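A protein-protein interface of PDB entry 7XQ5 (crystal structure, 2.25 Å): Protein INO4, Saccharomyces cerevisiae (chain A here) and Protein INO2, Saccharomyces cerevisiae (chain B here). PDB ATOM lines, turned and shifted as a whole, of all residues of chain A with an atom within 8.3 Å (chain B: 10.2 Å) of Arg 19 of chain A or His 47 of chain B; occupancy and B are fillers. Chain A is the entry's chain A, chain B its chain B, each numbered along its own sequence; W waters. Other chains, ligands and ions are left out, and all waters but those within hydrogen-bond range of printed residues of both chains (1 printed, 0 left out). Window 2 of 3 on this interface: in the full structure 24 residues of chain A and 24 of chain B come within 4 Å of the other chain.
NZ of Lys 46 of chain B lies within hydrogen-bond range of OH of Tyr 49 of chain A (3.3 Å).
NH2 of Arg 19 of chain A is in salt-bridge range of OE2 of Glu 16 of chain A (2.8 Å).
The backbone carbonyl oxygen (O) of Thr 51 of chain B sits close to the side-chain amide nitrogen (ND2) of Asn 55 of chain B (3.4 Å).
The guanidinium group (NE) of Arg 19 of chain A is in salt-bridge range of the side-chain carboxylate (OE2) of Glu 23 of chain A (3.0 Å).
OG1 of Thr 51 of chain B is in hydrogen-bond range of O of His 47 of chain B (3.0 Å).
His 47 of chain B touches Arg 19 of chain A (CD2 to CG, 3.9 Å).
Leu 22 of chain A touches His 47 of chain B (CD2 to ND1, 3.9 Å).
Glu 23 of chain A touches His 47 of chain B (CG to CB, 3.9 Å).
Ile 26 of chain A touches His 47 of chain B.
Ile 26 of chain A touches Leu 50 of chain B (CG2 to CB, 3.8 Å).
CD1 of Ile 26 of chain A touches OG1 of Thr 51 of chain B, at 3.97 Å.
CE1 of Phe 27 of chain A touches CD1 of Leu 50 of chain B (3.7 Å).
Phe 26 of chain B touches Tyr 49 of chain A (CB to CD2, 3.6 Å).
Tyr 49 of chain A touches Leu 50 of chain B (CE1 to CD2, 3.7 Å).
Of chain B, only His 47 (3.9 Å) comes within 4 Å of Arg 19 of chain A.
His 47 of chain B touches just these residues of chain A: Arg 19, Leu 22, Glu 23 and Ile 26.
No residue of chain B comes within 4 Å of Glu 16 of chain A.
Of chain B, only His 47 (3.9 Å) comes within 4 Å of Leu 22 of chain A.
Of chain B, only His 47 (3.9 Å) comes within 4 Å of Glu 23 of chain A.
Of the printed residues of chain B, Tyr 49 of chain A touches Phe 26 (3.6 Å), Lys 46 (3.3 Å) and Leu 50 (3.7 Å).
Of the printed residues of chain A, Lys 46 of chain B touches Tyr 49 (3.3 Å).
Printed residues of chain A within 4 Å of Thr 51 of chain B: Ile 26.
Printed residues of chain B within 4 Å of Ile 26 of chain A: His 47 (3.9 Å), Leu 50 (3.8 Å) and Thr 51 (3.97 Å).
Of the printed residues of chain A, Phe 26 of chain B touches Tyr 49.
Val 13 of chain A touches none of the printed residues of chain B.
Ile 48 of chain B touches none of the printed residues of chain A.
The nearest residue of chain B that does not touch Arg 19 of chain A is Pro 45 of chain B (5.8 Å).
Of the 17 printed residues of chain A, 6 touch a printed residue of chain B.
Of the 18 printed residues of chain B, 5 touch a printed residue of chain A.
Hydrophobic or aromatic side chains of chain B that line the printed part of chain A: Phe 26, His 47 and Leu 50.
Water W1 bridges the side-chain carboxylate of Glu 23 of chain A and the backbone NH of His 47 of chain B.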
ATOM      1  N   HIS A  12      -8.340 -20.570  26.500  1.00  0.00           N
ATOM      2  CA  HIS A  12      -8.629 -21.999  26.382  1.00  0.00           C
ATOM      3  C   HIS A  12     -10.125 -22.258  26.543  1.00  0.00           C
ATOM      4  O   HIS A  12     -10.757 -22.895  25.689  1.00  0.00           O
ATOM      5  CB  HIS A  12      -7.802 -22.738  27.438  1.00  0.00           C
ATOM      6  CG  HIS A  12      -7.919 -24.228  27.416  1.00  0.00           C
ATOM      7  ND1 HIS A  12      -8.553 -24.925  26.411  1.00  0.00           N
ATOM      8  CD2 HIS A  12      -7.440 -25.160  28.274  1.00  0.00           C
ATOM      9  CE1 HIS A  12      -8.473 -26.223  26.657  1.00  0.00           C
ATOM     10  NE2 HIS A  12      -7.806 -26.389  27.785  1.00  0.00           N
ATOM     11  N   VAL A  13     -10.728 -21.708  27.604  1.00  0.00           N
ATOM     12  CA  VAL A  13     -12.161 -21.914  27.829  1.00  0.00           C
ATOM     13  C   VAL A  13     -12.977 -21.382  26.653  1.00  0.00           C
ATOM     14  O   VAL A  13     -13.863 -22.068  26.124  1.00  0.00           O
ATOM     15  CB  VAL A  13     -12.595 -21.258  29.149  1.00  0.00           C
ATOM     16  CG1 VAL A  13     -14.117 -21.297  29.266  1.00  0.00           C
ATOM     17  CG2 VAL A  13     -11.912 -21.934  30.326  1.00  0.00           C
ATOM     18  N   SER A  14     -12.697 -20.150  26.223  1.00  0.00           N
ATOM     19  CA  SER A  14     -13.488 -19.569  25.142  1.00  0.00           C
ATOM     20  C   SER A  14     -13.306 -20.321  23.836  1.00  0.00           C
ATOM     21  O   SER A  14     -14.241 -20.408  23.031  1.00  0.00           O
ATOM     22  CB  SER A  14     -13.116 -18.105  24.953  1.00  0.00           C
ATOM     23  OG  SER A  14     -13.151 -17.444  26.205  1.00  0.00           O
ATOM     24  N   SER A  15     -12.120 -20.861  23.591  1.00  0.00           N
ATOM     25  CA  SER A  15     -11.937 -21.611  22.354  1.00  0.00           C
ATOM     26  C   SER A  15     -12.798 -22.860  22.359  1.00  0.00           C
ATOM     27  O   SER A  15     -13.412 -23.205  21.344  1.00  0.00           O
ATOM     28  CB  SER A  15     -10.476 -21.995  22.179  1.00  0.00           C
ATOM     29  OG  SER A  15     -10.337 -22.693  20.958  1.00  0.00           O
ATOM     30  N   GLU A  16     -12.842 -23.552  23.501  1.00  0.00           N
ATOM     31  CA  GLU A  16     -13.698 -24.725  23.647  1.00  0.00           C
ATOM     32  C   GLU A  16     -15.163 -24.337  23.512  1.00  0.00           C
ATOM     33  O   GLU A  16     -15.921 -24.944  22.745  1.00  0.00           O
ATOM     34  CB  GLU A  16     -13.420 -25.386  25.005  1.00  0.00           C
ATOM     35  CG  GLU A  16     -14.163 -26.692  25.264  1.00  0.00           C
ATOM     36  CD  GLU A  16     -13.610 -27.851  24.448  1.00  0.00           C
ATOM     37  OE1 GLU A  16     -12.457 -27.743  23.971  1.00  0.00           O
ATOM     38  OE2 GLU A  16     -14.335 -28.860  24.263  1.00  0.00           O
ATOM     39  N   LYS A  17     -15.571 -23.294  24.223  1.00  0.00           N
ATOM     40  CA  LYS A  17     -16.962 -22.861  24.177  1.00  0.00           C
ATOM     41  C   LYS A  17     -17.398 -22.531  22.756  1.00  0.00           C
ATOM     42  O   LYS A  17     -18.466 -22.962  22.305  1.00  0.00           O
ATOM     43  CB  LYS A  17     -17.138 -21.665  25.104  1.00  0.00           C
ATOM     44  CG  LYS A  17     -18.559 -21.225  25.295  1.00  0.00           C
ATOM     45  CD  LYS A  17     -18.679 -20.338  26.534  1.00  0.00           C
ATOM     46  CE  LYS A  17     -18.415 -21.152  27.803  1.00  0.00           C
ATOM     47  NZ  LYS A  17     -19.043 -20.526  29.004  1.00  0.00           N
ATOM     48  N   LYS A  18     -16.584 -21.770  22.023  1.00  0.00           N
ATOM     49  CA  LYS A  18     -16.972 -21.390  20.666  1.00  0.00           C
ATOM     50  C   LYS A  18     -17.133 -22.608  19.766  1.00  0.00           C
ATOM     51  O   LYS A  18     -18.074 -22.680  18.960  1.00  0.00           O
ATOM     52  CB  LYS A  18     -15.949 -20.419  20.079  1.00  0.00           C
ATOM     53  CG  LYS A  18     -15.972 -19.071  20.788  1.00  0.00           C
ATOM     54  CD  LYS A  18     -15.490 -17.912  19.913  1.00  0.00           C
ATOM     55  CE  LYS A  18     -15.552 -16.575  20.680  1.00  0.00           C
ATOM     56  NZ  LYS A  18     -16.972 -16.074  20.893  1.00  0.00           N
ATOM     57  N   ARG A  19     -16.228 -23.575  19.877  1.00  0.00           N
ATOM     58  CA  ARG A  19     -16.361 -24.762  19.046  1.00  0.00           C
ATOM     59  C   ARG A  19     -17.614 -25.557  19.408  1.00  0.00           C
ATOM     60  O   ARG A  19     -18.322 -26.039  18.509  1.00  0.00           O
ATOM     61  CB  ARG A  19     -15.114 -25.628  19.160  1.00  0.00           C
ATOM     62  CG  ARG A  19     -15.027 -26.673  18.046  1.00  0.00           C
ATOM     63  CD  ARG A  19     -13.980 -27.749  18.364  1.00  0.00           C
ATOM     64  NE  ARG A  19     -14.442 -28.643  19.421  1.00  0.00           N
ATOM     65  CZ  ARG A  19     -14.001 -28.608  20.670  1.00  0.00           C
ATOM     66  NH1 ARG A  19     -13.049 -27.775  21.032  1.00  0.00           N
ATOM     67  NH2 ARG A  19     -14.527 -29.436  21.578  1.00  0.00           N
ATOM     68  N   ARG A  20     -17.921 -25.697  20.709  1.00  0.00           N
ATOM     69  CA  ARG A  20     -19.170 -26.375  21.084  1.00  0.00           C
ATOM     70  C   ARG A  20     -20.366 -25.635  20.517  1.00  0.00           C
ATOM     71  O   ARG A  20     -21.283 -26.251  19.955  1.00  0.00           O
ATOM     72  CB  ARG A  20     -19.314 -26.498  22.604  1.00  0.00           C
ATOM     73  CG  ARG A  20     -18.426 -27.534  23.258  1.00  0.00           C
ATOM     74  CD  ARG A  20     -18.819 -27.765  24.728  1.00  0.00           C
ATOM     75  NE  ARG A  20     -18.930 -26.533  25.507  1.00  0.00           N
ATOM     76  CZ  ARG A  20     -18.166 -26.231  26.549  1.00  0.00           C
ATOM     77  NH1 ARG A  20     -17.232 -27.057  26.980  1.00  0.00           N
ATOM     78  NH2 ARG A  20     -18.355 -25.073  27.179  1.00  0.00           N
ATOM     79  N   GLU A  21     -20.364 -24.306  20.627  1.00  0.00           N
ATOM     80  CA  GLU A  21     -21.466 -23.533  20.058  1.00  0.00           C
ATOM     81  C   GLU A  21     -21.561 -23.749  18.552  1.00  0.00           C
ATOM     82  O   GLU A  21     -22.660 -23.845  17.999  1.00  0.00           O
ATOM     83  CB  GLU A  21     -21.295 -22.054  20.421  1.00  0.00           C
ATOM     84  CG  GLU A  21     -21.552 -21.778  21.909  1.00  0.00           C
ATOM     85  CD  GLU A  21     -21.126 -20.378  22.384  1.00  0.00           C
ATOM     86  OE1 GLU A  21     -20.526 -19.607  21.590  1.00  0.00           O
ATOM     87  OE2 GLU A  21     -21.386 -20.054  23.572  1.00  0.00           O
ATOM     88  N   LEU A  22     -20.418 -23.892  17.884  1.00  0.00           N
ATOM     89  CA  LEU A  22     -20.407 -24.170  16.448  1.00  0.00           C
ATOM     90  C   LEU A  22     -21.013 -25.534  16.142  1.00  0.00           C
ATOM     91  O   LEU A  22     -21.824 -25.680  15.217  1.00  0.00           O
ATOM     92  CB  LEU A  22     -18.968 -24.104  15.936  1.00  0.00           C
ATOM     93  CG  LEU A  22     -18.645 -23.833  14.473  1.00  0.00           C
ATOM     94  CD1 LEU A  22     -19.432 -22.643  13.974  1.00  0.00           C
ATOM     95  CD2 LEU A  22     -17.151 -23.562  14.353  1.00  0.00           C
ATOM     96  N   GLU A  23     -20.609 -26.549  16.899  1.00  0.00           N
ATOM     97  CA  GLU A  23     -21.144 -27.890  16.694  1.00  0.00           C
ATOM     98  C   GLU A  23     -22.645 -27.908  16.935  1.00  0.00           C
ATOM     99  O   GLU A  23     -23.414 -28.407  16.109  1.00  0.00           O
ATOM    100  CB  GLU A  23     -20.407 -28.876  17.609  1.00  0.00           C
ATOM    101  CG  GLU A  23     -18.920 -29.049  17.211  1.00  0.00           C
ATOM    102  CD  GLU A  23     -18.074 -29.721  18.279  1.00  0.00           C
ATOM    103  OE1 GLU A  23     -18.636 -30.144  19.318  1.00  0.00           O
ATOM    104  OE2 GLU A  23     -16.835 -29.827  18.090  1.00  0.00           O
ATOM    105  N   ARG A  24     -23.082 -27.299  18.034  1.00  0.00           N
ATOM    106  CA  ARG A  24     -24.502 -27.296  18.362  1.00  0.00           C
ATOM    107  C   ARG A  24     -25.322 -26.663  17.258  1.00  0.00           C
ATOM    108  O   ARG A  24     -26.398 -27.162  16.917  1.00  0.00           O
ATOM    109  CB  ARG A  24     -24.730 -26.573  19.689  1.00  0.00           C
ATOM    110  CG  ARG A  24     -24.309 -27.416  20.859  1.00  0.00           C
ATOM    111  CD  ARG A  24     -24.055 -26.592  22.098  1.00  0.00           C
ATOM    112  NE  ARG A  24     -23.476 -27.440  23.133  1.00  0.00           N
ATOM    113  CZ  ARG A  24     -23.019 -26.991  24.291  1.00  0.00           C
ATOM    114  NH1 ARG A  24     -23.122 -25.715  24.623  1.00  0.00           N
ATOM    115  NH2 ARG A  24     -22.428 -27.838  25.129  1.00  0.00           N
ATOM    116  N   ALA A  25     -24.832 -25.565  16.676  1.00  0.00           N
ATOM    117  CA  ALA A  25     -25.564 -24.941  15.579  1.00  0.00           C
ATOM    118  C   ALA A  25     -25.753 -25.918  14.431  1.00  0.00           C
ATOM    119  O   ALA A  25     -26.824 -25.957  13.811  1.00  0.00           O
ATOM    120  CB  ALA A  25     -24.843 -23.682  15.095  1.00  0.00           C
ATOM    121  N   ILE A  26     -24.740 -26.740  14.150  1.00  0.00           N
ATOM    122  CA  ILE A  26     -24.897 -27.726  13.086  1.00  0.00           C
ATOM    123  C   ILE A  26     -25.866 -28.813  13.507  1.00  0.00           C
ATOM    124  O   ILE A  26     -26.696 -29.255  12.706  1.00  0.00           O
ATOM    125  CB  ILE A  26     -23.539 -28.300  12.662  1.00  0.00           C
ATOM    126  CG1 ILE A  26     -22.692 -27.176  12.069  1.00  0.00           C
ATOM    127  CG2 ILE A  26     -23.732 -29.372  11.607  1.00  0.00           C
ATOM    128  CD1 ILE A  26     -21.205 -27.419  12.127  1.00  0.00           C
ATOM    129  N   PHE A  27     -25.805 -29.248  14.774  1.00  0.00           N
ATOM    130  CA  PHE A  27     -26.811 -30.190  15.261  1.00  0.00           C
ATOM    131  C   PHE A  27     -28.207 -29.669  14.962  1.00  0.00           C
ATOM    132  O   PHE A  27     -29.061 -30.411  14.456  1.00  0.00           O
ATOM    133  CB  PHE A  27     -26.669 -30.448  16.769  1.00  0.00           C
ATOM    134  CG  PHE A  27     -25.361 -31.106  17.182  1.00  0.00           C
ATOM    135  CD1 PHE A  27     -24.574 -31.795  16.263  1.00  0.00           C
ATOM    136  CD2 PHE A  27     -24.932 -31.029  18.498  1.00  0.00           C
ATOM    137  CE1 PHE A  27     -23.383 -32.398  16.653  1.00  0.00           C
ATOM    138  CE2 PHE A  27     -23.741 -31.612  18.906  1.00  0.00           C
ATOM    139  CZ  PHE A  27     -22.960 -32.301  17.977  1.00  0.00           C
ATOM    140  N   TYR A  49     -26.120 -38.757  14.761  1.00  0.00           N
ATOM    141  CA  TYR A  49     -25.287 -39.407  13.755  1.00  0.00           C
ATOM    142  C   TYR A  49     -26.008 -40.593  13.139  1.00  0.00           C
ATOM    143  O   TYR A  49     -26.015 -40.751  11.917  1.00  0.00           O
ATOM    144  CB  TYR A  49     -23.941 -39.822  14.369  1.00  0.00           C
ATOM    145  CG  TYR A  49     -23.173 -38.650  14.967  1.00  0.00           C
ATOM    146  CD1 TYR A  49     -23.423 -37.351  14.539  1.00  0.00           C
ATOM    147  CD2 TYR A  49     -22.203 -38.838  15.943  1.00  0.00           C
ATOM    148  CE1 TYR A  49     -22.746 -36.272  15.066  1.00  0.00           C
ATOM    149  CE2 TYR A  49     -21.514 -37.757  16.474  1.00  0.00           C
ATOM    150  CZ  TYR A  49     -21.801 -36.471  16.026  1.00  0.00           C
ATOM    151  OH  TYR A  49     -21.144 -35.364  16.531  1.00  0.00           O
ATOM    152  N   PHE B  26     -20.270 -41.930  14.739  1.00  0.00           N
ATOM    153  CA  PHE B  26     -19.749 -40.822  13.949  1.00  0.00           C
ATOM    154  C   PHE B  26     -18.872 -41.333  12.815  1.00  0.00           C
ATOM    155  O   PHE B  26     -18.989 -40.881  11.669  1.00  0.00           O
ATOM    156  CB  PHE B  26     -18.963 -39.881  14.854  1.00  0.00           C
ATOM    157  CG  PHE B  26     -18.434 -38.652  14.159  1.00  0.00           C
ATOM    158  CD1 PHE B  26     -19.295 -37.718  13.624  1.00  0.00           C
ATOM    159  CD2 PHE B  26     -17.074 -38.415  14.087  1.00  0.00           C
ATOM    160  CE1 PHE B  26     -18.817 -36.589  13.014  1.00  0.00           C
ATOM    161  CE2 PHE B  26     -16.587 -37.282  13.475  1.00  0.00           C
ATOM    162  CZ  PHE B  26     -17.456 -36.366  12.950  1.00  0.00           C
ATOM    163  N   ILE B  30     -19.397 -40.751   8.889  1.00  0.00           N
ATOM    164  CA  ILE B  30     -18.419 -40.037   8.076  1.00  0.00           C
ATOM    165  C   ILE B  30     -17.872 -40.906   6.942  1.00  0.00           C
ATOM    166  O   ILE B  30     -17.502 -40.389   5.886  1.00  0.00           O
ATOM    167  CB  ILE B  30     -17.300 -39.515   8.983  1.00  0.00           C
ATOM    168  CG1 ILE B  30     -17.841 -38.381   9.839  1.00  0.00           C
ATOM    169  CG2 ILE B  30     -16.155 -39.013   8.175  1.00  0.00           C
ATOM    170  CD1 ILE B  30     -18.507 -37.290   9.026  1.00  0.00           C
ATOM    171  N   VAL B  33     -19.660 -40.163   3.718  1.00  0.00           N
ATOM    172  CA  VAL B  33     -19.783 -38.742   3.434  1.00  0.00           C
ATOM    173  C   VAL B  33     -18.569 -38.316   2.627  1.00  0.00           C
ATOM    174  O   VAL B  33     -17.442 -38.711   2.945  1.00  0.00           O
ATOM    175  CB  VAL B  33     -19.907 -37.940   4.745  1.00  0.00           C
ATOM    176  CG1 VAL B  33     -19.572 -36.491   4.565  1.00  0.00           C
ATOM    177  CG2 VAL B  33     -21.315 -38.104   5.288  1.00  0.00           C
ATOM    178  N   THR B  35     -15.699 -36.459   2.106  1.00  0.00           N
ATOM    179  CA  THR B  35     -14.899 -35.618   2.972  1.00  0.00           C
ATOM    180  C   THR B  35     -13.660 -35.108   2.237  1.00  0.00           C
ATOM    181  O   THR B  35     -13.185 -35.754   1.296  1.00  0.00           O
ATOM    182  CB  THR B  35     -14.473 -36.392   4.227  1.00  0.00           C
ATOM    183  OG1 THR B  35     -13.976 -37.684   3.855  1.00  0.00           O
ATOM    184  CG2 THR B  35     -15.656 -36.564   5.158  1.00  0.00           C
ATOM    185  N   PRO B  36     -13.115 -33.956   2.637  1.00  0.00           N
ATOM    186  CA  PRO B  36     -11.961 -33.414   1.923  1.00  0.00           C
ATOM    187  C   PRO B  36     -10.767 -34.326   2.065  1.00  0.00           C
ATOM    188  O   PRO B  36     -10.587 -34.998   3.100  1.00  0.00           O
ATOM    189  CB  PRO B  36     -11.718 -32.061   2.614  1.00  0.00           C
ATOM    190  CG  PRO B  36     -12.943 -31.759   3.379  1.00  0.00           C
ATOM    191  CD  PRO B  36     -13.519 -33.087   3.758  1.00  0.00           C
ATOM    192  N   ARG B  43      -5.441 -33.944  10.709  1.00  0.00           N
ATOM    193  CA  ARG B  43      -6.787 -34.387  11.050  1.00  0.00           C
ATOM    194  C   ARG B  43      -7.798 -33.317  10.671  1.00  0.00           C
ATOM    195  O   ARG B  43      -7.481 -32.128  10.597  1.00  0.00           O
ATOM    196  CB  ARG B  43      -6.907 -34.710  12.538  1.00  0.00           C
ATOM    197  CG  ARG B  43      -7.149 -33.494  13.419  1.00  0.00           C
ATOM    198  CD  ARG B  43      -7.282 -33.882  14.877  1.00  0.00           C
ATOM    199  NE  ARG B  43      -7.034 -32.741  15.748  1.00  0.00           N
ATOM    200  CZ  ARG B  43      -6.811 -32.827  17.052  1.00  0.00           C
ATOM    201  NH1 ARG B  43      -6.824 -33.995  17.682  1.00  0.00           N
ATOM    202  NH2 ARG B  43      -6.556 -31.717  17.741  1.00  0.00           N
ATOM    203  N   ILE B  44      -9.019 -33.749  10.394  1.00  0.00           N
ATOM    204  CA  ILE B  44     -10.120 -32.842  10.093  1.00  0.00           C
ATOM    205  C   ILE B  44     -10.979 -32.732  11.345  1.00  0.00           C
ATOM    206  O   ILE B  44     -11.478 -33.759  11.832  1.00  0.00           O
ATOM    207  CB  ILE B  44     -10.946 -33.328   8.897  1.00  0.00           C
ATOM    208  CG1 ILE B  44     -10.030 -33.635   7.713  1.00  0.00           C
ATOM    209  CG2 ILE B  44     -11.927 -32.257   8.480  1.00  0.00           C
ATOM    210  CD1 ILE B  44     -10.792 -34.127   6.509  1.00  0.00           C
ATOM    211  N   PRO B  45     -11.154 -31.541  11.908  1.00  0.00           N
ATOM    212  CA  PRO B  45     -11.954 -31.406  13.127  1.00  0.00           C
ATOM    213  C   PRO B  45     -13.384 -31.867  12.893  1.00  0.00           C
ATOM    214  O   PRO B  45     -13.922 -31.742  11.786  1.00  0.00           O
ATOM    215  CB  PRO B  45     -11.899 -29.904  13.420  1.00  0.00           C
ATOM    216  CG  PRO B  45     -10.689 -29.406  12.664  1.00  0.00           C
ATOM    217  CD  PRO B  45     -10.601 -30.256  11.448  1.00  0.00           C
ATOM    218  N   LYS B  46     -13.996 -32.399  13.961  1.00  0.00           N
ATOM    219  CA  LYS B  46     -15.371 -32.897  13.879  1.00  0.00           C
ATOM    220  C   LYS B  46     -16.297 -31.891  13.213  1.00  0.00           C
ATOM    221  O   LYS B  46     -17.104 -32.251  12.346  1.00  0.00           O
ATOM    222  CB  LYS B  46     -15.921 -33.239  15.270  1.00  0.00           C
ATOM    223  CG  LYS B  46     -17.382 -33.725  15.221  1.00  0.00           C
ATOM    224  CD  LYS B  46     -18.137 -33.590  16.544  1.00  0.00           C
ATOM    225  CE  LYS B  46     -17.527 -34.404  17.647  1.00  0.00           C
ATOM    226  NZ  LYS B  46     -18.014 -35.807  17.631  1.00  0.00           N
ATOM    227  N   HIS B  47     -16.214 -30.619  13.610  1.00  0.00           N
ATOM    228  CA  HIS B  47     -17.188 -29.669  13.079  1.00  0.00           C
ATOM    229  C   HIS B  47     -17.006 -29.456  11.581  1.00  0.00           C
ATOM    230  O   HIS B  47     -17.980 -29.157  10.878  1.00  0.00           O
ATOM    231  CB  HIS B  47     -17.117 -28.339  13.830  1.00  0.00           C
ATOM    232  CG  HIS B  47     -15.889 -27.534  13.542  1.00  0.00           C
ATOM    233  ND1 HIS B  47     -15.801 -26.665  12.473  1.00  0.00           N
ATOM    234  CD2 HIS B  47     -14.701 -27.458  14.189  1.00  0.00           C
ATOM    235  CE1 HIS B  47     -14.608 -26.096  12.469  1.00  0.00           C
ATOM    236  NE2 HIS B  47     -13.922 -26.556  13.502  1.00  0.00           N
ATOM    237  N   ILE B  48     -15.781 -29.597  11.067  1.00  0.00           N
ATOM    238  CA  ILE B  48     -15.620 -29.539   9.617  1.00  0.00           C
ATOM    239  C   ILE B  48     -16.317 -30.726   8.990  1.00  0.00           C
ATOM    240  O   ILE B  48     -17.050 -30.588   8.006  1.00  0.00           O
ATOM    241  CB  ILE B  48     -14.137 -29.496   9.205  1.00  0.00           C
ATOM    242  CG1 ILE B  48     -13.440 -28.243   9.740  1.00  0.00           C
ATOM    243  CG2 ILE B  48     -14.038 -29.517   7.689  1.00  0.00           C
ATOM    244  CD1 ILE B  48     -13.843 -26.966   9.022  1.00  0.00           C
ATOM    245  N   LEU B  49     -16.123 -31.908   9.570  1.00  0.00           N
ATOM    246  CA  LEU B  49     -16.799 -33.092   9.067  1.00  0.00           C
ATOM    247  C   LEU B  49     -18.310 -32.919   9.133  1.00  0.00           C
ATOM    248  O   LEU B  49     -19.029 -33.346   8.224  1.00  0.00           O
ATOM    249  CB  LEU B  49     -16.341 -34.317   9.859  1.00  0.00           C
ATOM    250  CG  LEU B  49     -14.837 -34.545   9.692  1.00  0.00           C
ATOM    251  CD1 LEU B  49     -14.316 -35.662  10.583  1.00  0.00           C
ATOM    252  CD2 LEU B  49     -14.566 -34.845   8.233  1.00  0.00           C
ATOM    253  N   LEU B  50     -18.814 -32.260  10.177  1.00  0.00           N
ATOM    254  CA  LEU B  50     -20.266 -32.111  10.276  1.00  0.00           C
ATOM    255  C   LEU B  50     -20.796 -31.235   9.151  1.00  0.00           C
ATOM    256  O   LEU B  50     -21.886 -31.480   8.627  1.00  0.00           O
ATOM    257  CB  LEU B  50     -20.659 -31.538  11.639  1.00  0.00           C
ATOM    258  CG  LEU B  50     -20.495 -32.448  12.869  1.00  0.00           C
ATOM    259  CD1 LEU B  50     -20.781 -31.679  14.160  1.00  0.00           C
ATOM    260  CD2 LEU B  50     -21.395 -33.668  12.777  1.00  0.00           C
ATOM    261  N   THR B  51     -20.037 -30.213   8.759  1.00  0.00           N
ATOM    262  CA  THR B  51     -20.439 -29.402   7.613  1.00  0.00           C
ATOM    263  C   THR B  51     -20.525 -30.250   6.348  1.00  0.00           C
ATOM    264  O   THR B  51     -21.446 -30.088   5.537  1.00  0.00           O
ATOM    265  CB  THR B  51     -19.450 -28.255   7.423  1.00  0.00           C
ATOM    266  OG1 THR B  51     -19.236 -27.596   8.685  1.00  0.00           O
ATOM    267  CG2 THR B  51     -19.988 -27.256   6.408  1.00  0.00           C
ATOM    268  N   CYS B  52     -19.583 -31.175   6.168  1.00  0.00           N
ATOM    269  CA  CYS B  52     -19.650 -32.073   5.021  1.00  0.00           C
ATOM    270  C   CYS B  52     -20.913 -32.910   5.057  1.00  0.00           C
ATOM    271  O   CYS B  52     -21.522 -33.167   4.012  1.00  0.00           O
ATOM    272  CB  CYS B  52     -18.418 -32.962   4.981  1.00  0.00           C
ATOM    273  SG  CYS B  52     -16.917 -32.027   4.717  1.00  0.00           S
ATOM    274  N   VAL B  53     -21.334 -33.334   6.255  1.00  0.00           N
ATOM    275  CA  VAL B  53     -22.594 -34.057   6.378  1.00  0.00           C
ATOM    276  C   VAL B  53     -23.740 -33.210   5.849  1.00  0.00           C
ATOM    277  O   VAL B  53     -24.495 -33.639   4.972  1.00  0.00           O
ATOM    278  CB  VAL B  53     -22.847 -34.478   7.833  1.00  0.00           C
ATOM    279  CG1 VAL B  53     -24.223 -35.102   7.940  1.00  0.00           C
ATOM    280  CG2 VAL B  53     -21.772 -35.447   8.321  1.00  0.00           C
ATOM    281  N   MET B  54     -23.887 -31.991   6.377  1.00  0.00           N
ATOM    282  CA  MET B  54     -24.987 -31.128   5.940  1.00  0.00           C
ATOM    283  C   MET B  54     -24.948 -30.901   4.437  1.00  0.00           C
ATOM    284  O   MET B  54     -25.986 -30.984   3.767  1.00  0.00           O
ATOM    285  CB  MET B  54     -24.941 -29.786   6.673  1.00  0.00           C
ATOM    286  CG  MET B  54     -25.699 -29.751   8.004  1.00  0.00           C
ATOM    287  SD  MET B  54     -27.447 -30.116   7.779  1.00  0.00           S
ATOM    288  CE  MET B  54     -27.838 -28.929   6.494  1.00  0.00           C
ATOM    289  N   ASN B  55     -23.758 -30.619   3.889  1.00  0.00           N
ATOM    290  CA  ASN B  55     -23.620 -30.435   2.444  1.00  0.00           C
ATOM    291  C   ASN B  55     -24.133 -31.652   1.685  1.00  0.00           C
ATOM    292  O   ASN B  55     -24.976 -31.524   0.790  1.00  0.00           O
ATOM    293  CB  ASN B  55     -22.164 -30.164   2.073  1.00  0.00           C
ATOM    294  CG  ASN B  55     -21.656 -28.844   2.609  1.00  0.00           C
ATOM    295  OD1 ASN B  55     -22.436 -27.957   2.986  1.00  0.00           O
ATOM    296  ND2 ASN B  55     -20.333 -28.694   2.629  1.00  0.00           N
HETATM  297  O   HOH W   1     -15.252 -29.950  16.182  1.00  0.00           O
